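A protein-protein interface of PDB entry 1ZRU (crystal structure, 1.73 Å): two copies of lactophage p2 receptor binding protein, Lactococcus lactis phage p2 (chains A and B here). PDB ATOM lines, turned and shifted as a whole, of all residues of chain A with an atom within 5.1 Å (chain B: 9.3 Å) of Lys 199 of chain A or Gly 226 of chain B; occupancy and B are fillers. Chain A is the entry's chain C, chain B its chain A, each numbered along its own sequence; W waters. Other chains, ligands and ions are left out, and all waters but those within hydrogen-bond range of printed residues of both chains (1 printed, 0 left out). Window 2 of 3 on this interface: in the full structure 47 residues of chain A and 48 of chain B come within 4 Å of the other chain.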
ATOM      1  N   ILE A 197      25.333  26.715  -5.078  1.00  0.00           N
ATOM      2  CA  ILE A 197      24.844  26.254  -6.390  1.00  0.00           C
ATOM      3  C   ILE A 197      24.075  24.934  -6.210  1.00  0.00           C
ATOM      4  O   ILE A 197      24.377  24.157  -5.302  1.00  0.00           O
ATOM      5  CB  ILE A 197      26.024  26.096  -7.389  1.00  0.00           C
ATOM      6  CG1 ILE A 197      25.522  25.795  -8.814  1.00  0.00           C
ATOM      7  CG2 ILE A 197      26.988  24.985  -6.934  1.00  0.00           C
ATOM      8  CD1 ILE A 197      25.345  26.964  -9.682  1.00  0.00           C
ATOM      9  N   GLN A 198      23.060  24.709  -7.044  1.00  0.00           N
ATOM     10  CA  GLN A 198      22.350  23.444  -7.044  1.00  0.00           C
ATOM     11  C   GLN A 198      22.604  22.726  -8.350  1.00  0.00           C
ATOM     12  O   GLN A 198      22.845  23.361  -9.374  1.00  0.00           O
ATOM     13  CB  GLN A 198      20.834  23.656  -6.937  1.00  0.00           C
ATOM     14  CG  GLN A 198      20.378  24.064  -5.561  1.00  0.00           C
ATOM     15  CD  GLN A 198      18.860  24.198  -5.454  1.00  0.00           C
ATOM     16  OE1 GLN A 198      18.086  23.621  -6.249  1.00  0.00           O
ATOM     17  NE2 GLN A 198      18.426  24.957  -4.461  1.00  0.00           N
ATOM     18  N   LYS A 199      22.483  21.406  -8.297  1.00  0.00           N
ATOM     19  CA  LYS A 199      22.536  20.575  -9.493  1.00  0.00           C
ATOM     20  C   LYS A 199      21.513  21.084 -10.508  1.00  0.00           C
ATOM     21  O   LYS A 199      20.367  21.406 -10.162  1.00  0.00           O
ATOM     22  CB  LYS A 199      22.282  19.115  -9.128  1.00  0.00           C
ATOM     23  CG  LYS A 199      20.903  18.838  -8.456  1.00  0.00           C
ATOM     24  CD  LYS A 199      20.811  17.387  -7.977  1.00  0.00           C
ATOM     25  CE  LYS A 199      21.376  17.228  -6.581  1.00  0.00           C
ATOM     26  NZ  LYS A 199      20.429  17.887  -5.599  1.00  0.00           N
ATOM     27  N   GLY A 200      21.941  21.197 -11.764  1.00  0.00           N
ATOM     28  CA  GLY A 200      21.046  21.620 -12.822  1.00  0.00           C
ATOM     29  C   GLY A 200      20.974  23.112 -13.083  1.00  0.00           C
ATOM     30  O   GLY A 200      20.464  23.529 -14.129  1.00  0.00           O
ATOM     31  N   TRP A 201      21.476  23.927 -12.149  1.00  0.00           N
ATOM     32  CA  TRP A 201      21.517  25.375 -12.352  1.00  0.00           C
ATOM     33  C   TRP A 201      22.635  25.755 -13.308  1.00  0.00           C
ATOM     34  O   TRP A 201      23.716  25.154 -13.273  1.00  0.00           O
ATOM     35  CB  TRP A 201      21.781  26.100 -11.033  1.00  0.00           C
ATOM     36  CG  TRP A 201      20.587  26.137 -10.105  1.00  0.00           C
ATOM     37  CD1 TRP A 201      19.379  25.514 -10.272  1.00  0.00           C
ATOM     38  CD2 TRP A 201      20.517  26.822  -8.850  1.00  0.00           C
ATOM     39  NE1 TRP A 201      18.550  25.783  -9.191  1.00  0.00           N
ATOM     40  CE2 TRP A 201      19.230  26.582  -8.307  1.00  0.00           C
ATOM     41  CE3 TRP A 201      21.411  27.634  -8.143  1.00  0.00           C
ATOM     42  CZ2 TRP A 201      18.823  27.120  -7.080  1.00  0.00           C
ATOM     43  CZ3 TRP A 201      21.007  28.164  -6.917  1.00  0.00           C
ATOM     44  CH2 TRP A 201      19.730  27.898  -6.401  1.00  0.00           C
ATOM     45  N   TRP A 243      25.872  23.338 -13.861  1.00  0.00           N
ATOM     46  CA  TRP A 243      26.482  22.606 -12.753  1.00  0.00           C
ATOM     47  C   TRP A 243      25.844  21.228 -12.573  1.00  0.00           C
ATOM     48  O   TRP A 243      24.622  21.119 -12.436  1.00  0.00           O
ATOM     49  CB  TRP A 243      26.317  23.398 -11.441  1.00  0.00           C
ATOM     50  CG  TRP A 243      26.918  22.697 -10.253  1.00  0.00           C
ATOM     51  CD1 TRP A 243      26.245  22.019  -9.252  1.00  0.00           C
ATOM     52  CD2 TRP A 243      28.311  22.591  -9.936  1.00  0.00           C
ATOM     53  NE1 TRP A 243      27.144  21.495  -8.349  1.00  0.00           N
ATOM     54  CE2 TRP A 243      28.415  21.843  -8.739  1.00  0.00           C
ATOM     55  CE3 TRP A 243      29.490  23.050 -10.555  1.00  0.00           C
ATOM     56  CZ2 TRP A 243      29.658  21.539  -8.150  1.00  0.00           C
ATOM     57  CZ3 TRP A 243      30.720  22.751  -9.965  1.00  0.00           C
ATOM     58  CH2 TRP A 243      30.791  22.001  -8.779  1.00  0.00           C
ATOM     59  N   TRP A 244      26.671  20.183 -12.553  1.00  0.00           N
ATOM     60  CA  TRP A 244      26.159  18.823 -12.338  1.00  0.00           C
ATOM     61  C   TRP A 244      26.866  18.061 -11.210  1.00  0.00           C
ATOM     62  O   TRP A 244      26.849  16.823 -11.161  1.00  0.00           O
ATOM     63  CB  TRP A 244      26.175  18.036 -13.664  1.00  0.00           C
ATOM     64  CG  TRP A 244      25.131  18.517 -14.619  1.00  0.00           C
ATOM     65  CD1 TRP A 244      25.347  19.144 -15.820  1.00  0.00           C
ATOM     66  CD2 TRP A 244      23.708  18.424 -14.463  1.00  0.00           C
ATOM     67  NE1 TRP A 244      24.136  19.453 -16.421  1.00  0.00           N
ATOM     68  CE2 TRP A 244      23.122  19.033 -15.604  1.00  0.00           C
ATOM     69  CE3 TRP A 244      22.868  17.891 -13.467  1.00  0.00           C
ATOM     70  CZ2 TRP A 244      21.731  19.111 -15.790  1.00  0.00           C
ATOM     71  CZ3 TRP A 244      21.490  17.978 -13.648  1.00  0.00           C
ATOM     72  CH2 TRP A 244      20.939  18.579 -14.806  1.00  0.00           C
ATOM     73  N   GLY A 245      27.490  18.798 -10.289  1.00  0.00           N
ATOM     74  CA  GLY A 245      27.871  18.204  -9.014  1.00  0.00           C
ATOM     75  C   GLY A 245      26.652  18.160  -8.085  1.00  0.00           C
ATOM     76  O   GLY A 245      25.519  18.507  -8.485  1.00  0.00           O
ATOM     77  N   ALA A 246      26.882  17.707  -6.857  1.00  0.00           N
ATOM     78  CA  ALA A 246      25.857  17.801  -5.798  1.00  0.00           C
ATOM     79  C   ALA A 246      25.638  19.272  -5.448  1.00  0.00           C
ATOM     80  O   ALA A 246      26.396  20.147  -5.868  1.00  0.00           O
ATOM     81  CB  ALA A 246      26.327  17.030  -4.557  1.00  0.00           C
ATOM     82  N   ASN A 247      24.601  19.564  -4.668  1.00  0.00           N
ATOM     83  CA  ASN A 247      24.372  20.955  -4.256  1.00  0.00           C
ATOM     84  C   ASN A 247      25.502  21.377  -3.335  1.00  0.00           C
ATOM     85  O   ASN A 247      25.957  20.569  -2.523  1.00  0.00           O
ATOM     86  CB  ASN A 247      23.057  21.081  -3.489  1.00  0.00           C
ATOM     87  CG  ASN A 247      21.843  20.729  -4.331  1.00  0.00           C
ATOM     88  OD1 ASN A 247      21.902  20.700  -5.550  1.00  0.00           O
ATOM     89  ND2 ASN A 247      20.728  20.456  -3.663  1.00  0.00           N
ATOM     90  N   HIS B 223      31.516  10.545 -14.213  1.00  0.00           N
ATOM     91  CA  HIS B 223      30.891  11.206 -13.049  1.00  0.00           C
ATOM     92  C   HIS B 223      29.399  10.906 -13.030  1.00  0.00           C
ATOM     93  O   HIS B 223      28.764  10.825 -14.081  1.00  0.00           O
ATOM     94  CB  HIS B 223      31.137  12.729 -13.076  1.00  0.00           C
ATOM     95  CG  HIS B 223      30.577  13.437 -11.879  1.00  0.00           C
ATOM     96  ND1 HIS B 223      29.479  14.265 -11.952  1.00  0.00           N
ATOM     97  CD2 HIS B 223      30.930  13.390 -10.571  1.00  0.00           C
ATOM     98  CE1 HIS B 223      29.171  14.695 -10.737  1.00  0.00           C
ATOM     99  NE2 HIS B 223      30.039  14.180  -9.883  1.00  0.00           N
ATOM    100  N   PHE B 224      28.841  10.745 -11.830  1.00  0.00           N
ATOM    101  CA  PHE B 224      27.411  10.566 -11.690  1.00  0.00           C
ATOM    102  C   PHE B 224      26.741  11.926 -11.562  1.00  0.00           C
ATOM    103  O   PHE B 224      27.015  12.669 -10.617  1.00  0.00           O
ATOM    104  CB  PHE B 224      27.118   9.710 -10.463  1.00  0.00           C
ATOM    105  CG  PHE B 224      27.562   8.268 -10.611  1.00  0.00           C
ATOM    106  CD1 PHE B 224      26.992   7.462 -11.593  1.00  0.00           C
ATOM    107  CD2 PHE B 224      28.541   7.734  -9.777  1.00  0.00           C
ATOM    108  CE1 PHE B 224      27.383   6.105 -11.733  1.00  0.00           C
ATOM    109  CE2 PHE B 224      28.948   6.380  -9.908  1.00  0.00           C
ATOM    110  CZ  PHE B 224      28.361   5.572 -10.887  1.00  0.00           C
ATOM    111  N   ALA B 225      25.869  12.250 -12.507  1.00  0.00           N
ATOM    112  CA  ALA B 225      25.242  13.591 -12.567  1.00  0.00           C
ATOM    113  C   ALA B 225      24.469  13.906 -11.288  1.00  0.00           C
ATOM    114  O   ALA B 225      23.721  13.067 -10.770  1.00  0.00           O
ATOM    115  CB  ALA B 225      24.333  13.721 -13.795  1.00  0.00           C
ATOM    116  N   GLY B 226      24.682  15.115 -10.781  1.00  0.00           N
ATOM    117  CA  GLY B 226      24.011  15.570  -9.560  1.00  0.00           C
ATOM    118  C   GLY B 226      24.524  14.993  -8.249  1.00  0.00           C
ATOM    119  O   GLY B 226      23.923  15.258  -7.193  1.00  0.00           O
ATOM    120  N   ARG B 227      25.623  14.224  -8.303  1.00  0.00           N
ATOM    121  CA  ARG B 227      26.234  13.586  -7.142  1.00  0.00           C
ATOM    122  C   ARG B 227      27.706  13.964  -6.937  1.00  0.00           C
ATOM    123  O   ARG B 227      28.328  14.589  -7.810  1.00  0.00           O
ATOM    124  CB  ARG B 227      26.146  12.051  -7.265  1.00  0.00           C
ATOM    125  CG  ARG B 227      24.730  11.544  -7.429  1.00  0.00           C
ATOM    126  CD  ARG B 227      24.697  10.063  -7.126  1.00  0.00           C
ATOM    127  NE  ARG B 227      23.321   9.636  -6.939  1.00  0.00           N
ATOM    128  CZ  ARG B 227      22.961   8.445  -6.484  1.00  0.00           C
ATOM    129  NH1 ARG B 227      21.672   8.166  -6.341  1.00  0.00           N
ATOM    130  NH2 ARG B 227      23.883   7.536  -6.186  1.00  0.00           N
ATOM    131  N   ASP B 228      28.251  13.569  -5.780  1.00  0.00           N
ATOM    132  CA  ASP B 228      29.687  13.729  -5.468  1.00  0.00           C
ATOM    133  C   ASP B 228      30.535  12.549  -5.936  1.00  0.00           C
ATOM    134  O   ASP B 228      31.740  12.529  -5.697  1.00  0.00           O
ATOM    135  CB  ASP B 228      29.870  13.722  -3.944  1.00  0.00           C
ATOM    136  CG  ASP B 228      29.569  15.020  -3.301  1.00  0.00           C
ATOM    137  OD1 ASP B 228      29.613  16.086  -3.966  1.00  0.00           O
ATOM    138  OD2 ASP B 228      29.312  14.958  -2.066  1.00  0.00           O
ATOM    139  N   THR B 229      29.900  11.545  -6.534  1.00  0.00           N
ATOM    140  CA  THR B 229      30.544  10.252  -6.729  1.00  0.00           C
ATOM    141  C   THR B 229      30.942  10.043  -8.194  1.00  0.00           C
ATOM    142  O   THR B 229      30.406  10.702  -9.089  1.00  0.00           O
ATOM    143  CB  THR B 229      29.605   9.127  -6.306  1.00  0.00           C
ATOM    144  OG1 THR B 229      28.320   9.336  -6.917  1.00  0.00           O
ATOM    145  CG2 THR B 229      29.464   9.109  -4.765  1.00  0.00           C
ATOM    146  N   ILE B 253      21.722   5.168 -12.124  1.00  0.00           N
ATOM    147  CA  ILE B 253      22.388   6.422 -11.784  1.00  0.00           C
ATOM    148  C   ILE B 253      22.946   6.977 -13.104  1.00  0.00           C
ATOM    149  O   ILE B 253      23.620   6.252 -13.848  1.00  0.00           O
ATOM    150  CB  ILE B 253      23.561   6.212 -10.765  1.00  0.00           C
ATOM    151  CG1 ILE B 253      23.141   5.325  -9.572  1.00  0.00           C
ATOM    152  CG2 ILE B 253      24.055   7.571 -10.203  1.00  0.00           C
ATOM    153  CD1 ILE B 253      24.312   4.949  -8.658  1.00  0.00           C
ATOM    154  N   ALA B 254      22.661   8.242 -13.384  1.00  0.00           N
ATOM    155  CA  ALA B 254      23.076   8.868 -14.642  1.00  0.00           C
ATOM    156  C   ALA B 254      24.587   9.028 -14.709  1.00  0.00           C
ATOM    157  O   ALA B 254      25.207   9.553 -13.792  1.00  0.00           O
ATOM    158  CB  ALA B 254      22.372  10.218 -14.831  1.00  0.00           C
ATOM    159  N   THR B 255      25.159   8.586 -15.831  1.00  0.00           N
ATOM    160  CA  THR B 255      26.614   8.544 -16.022  1.00  0.00           C
ATOM    161  C   THR B 255      27.013   9.544 -17.109  1.00  0.00           C
ATOM    162  O   THR B 255      26.451   9.520 -18.204  1.00  0.00           O
ATOM    163  CB  THR B 255      27.048   7.122 -16.467  1.00  0.00           C
ATOM    164  OG1 THR B 255      26.126   6.622 -17.460  1.00  0.00           O
ATOM    165  CG2 THR B 255      27.038   6.158 -15.280  1.00  0.00           C
ATOM    166  N   ARG B 256      28.010  10.386 -16.827  1.00  0.00           N
ATOM    167  CA  ARG B 256      28.405  11.444 -17.769  1.00  0.00           C
ATOM    168  C   ARG B 256      29.922  11.622 -17.725  1.00  0.00           C
ATOM    169  O   ARG B 256      30.592  11.121 -16.830  1.00  0.00           O
ATOM    170  CB  ARG B 256      27.742  12.786 -17.387  1.00  0.00           C
ATOM    171  CG  ARG B 256      26.200  12.819 -17.439  1.00  0.00           C
ATOM    172  CD  ARG B 256      25.671  12.749 -18.848  1.00  0.00           C
ATOM    173  NE  ARG B 256      24.207  12.829 -18.856  1.00  0.00           N
ATOM    174  CZ  ARG B 256      23.387  11.790 -18.701  1.00  0.00           C
ATOM    175  NH1 ARG B 256      23.862  10.563 -18.540  1.00  0.00           N
ATOM    176  NH2 ARG B 256      22.067  11.984 -18.712  1.00  0.00           N
HETATM  177  O   HOH W   1      29.625  17.308  -6.383  1.00  0.00           O
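N of Gly 226 of chain B sits at hydrogen-bond distance from O of Trp 244 of chain A.
The indole nitrogen (NE1) of Trp 243 of chain A lies close to the backbone carbonyl oxygen (O) of Gly 245 of chain A (3.4 Å). The backbone carbonyl oxygen of Ala 246 of chain A sits at hydrogen-bond distance from the indole nitrogen of Trp 243 of chain A (2.9 Å). O of Arg 227 of chain B is in hydrogen-bond range of NE2 of His 223 of chain B (2.7 Å). The backbone NH (N) of Lys 199 of chain A lies within hydrogen-bond range of the side-chain amide oxygen (OD1) of Asn 247 of chain A (2.9 Å). The backbone NH (N) of His 223 of chain B is in hydrogen-bond range of the backbone carbonyl oxygen (O) of Arg 256 of chain B. The backbone NH (N) of Ala 225 of chain B is in hydrogen-bond range of the backbone carbonyl oxygen (O) of Ala 254 of chain B (3.1 Å).
Gly 226 of chain B touches Lys 199 of chain A (O to CE, 3.3 Å). His 223 of chain B touches Trp 244 of chain A. O of Trp 244 of chain A touches C of Ala 225 of chain B, at 3.8 Å. O of Gly 245 of chain A touches CA of Gly 226 of chain B, 3.5 Å away. Gly 245 of chain A touches Arg 227 of chain B (CA to O, 3.8 Å). Ala 246 of chain A touches Gly 226 of chain B (CA to O, 3.5 Å). Ala 246 of chain A touches Arg 227 of chain B. OD1 of Asp 228 of chain B touches CB of Ala 246 of chain A (3.5 Å).
Lys 199 of chain A touches just one residue of chain B: Gly 226. No residue of chain B comes within 4 Å of Gly 200 of chain A. Printed residues of chain B within 4 Å of Trp 244 of chain A: His 223 (3.2 Å), Ala 225 (3.8 Å) and Gly 226 (2.8 Å). Printed residues of chain B within 4 Å of Ala 246 of chain A: Gly 226 (3.5 Å), Arg 227 (3.6 Å) and Asp 228 (3.5 Å). Asn 247 of chain A touches none of the printed residues of chain B. Of the printed residues of chain A, Ala 225 of chain B touches Trp 244 (3.8 Å). Gly 226 of chain B touches just these residues of chain A: Lys 199 (3.3 Å), Trp 244 (2.8 Å), Gly 245 (3.5 Å) and Ala 246 (3.5 Å). Of the printed residues of chain A, Asp 228 of chain B touches Ala 246. The nearest residue of chain B that does not touch Lys 199 of chain A is Arg 227 of chain B (5.5 Å). The nearest residue of chain A that does not touch Gly 226 of chain B is Asn 247 of chain A (5.0 Å). The nearest printed residue of chain A that does not touch Arg 227 of chain B is Trp 244 of chain A (4.1 Å).
Printed residues of chain A that touch a printed residue of chain B: Lys 199, Trp 244, Gly 245 and Ala 246. Hydrophobic or aromatic side chains of chain A that line the printed part of chain B: Ala 246. Of the 11 printed residues of chain B, 5 touch a printed residue of chain A.
No position is printed for both chains. Of the 9 pairs that touch across the chains among the printed residues, none has its exchanged pair printed and touching as well.
Water W1 lies within hydrogen-bond range of OD1 of Asp 228 of chain B (2.7 Å), N of Ala 246 of chain A (2.8 Å) and O of Arg 227 of chain B (3.3 Å).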
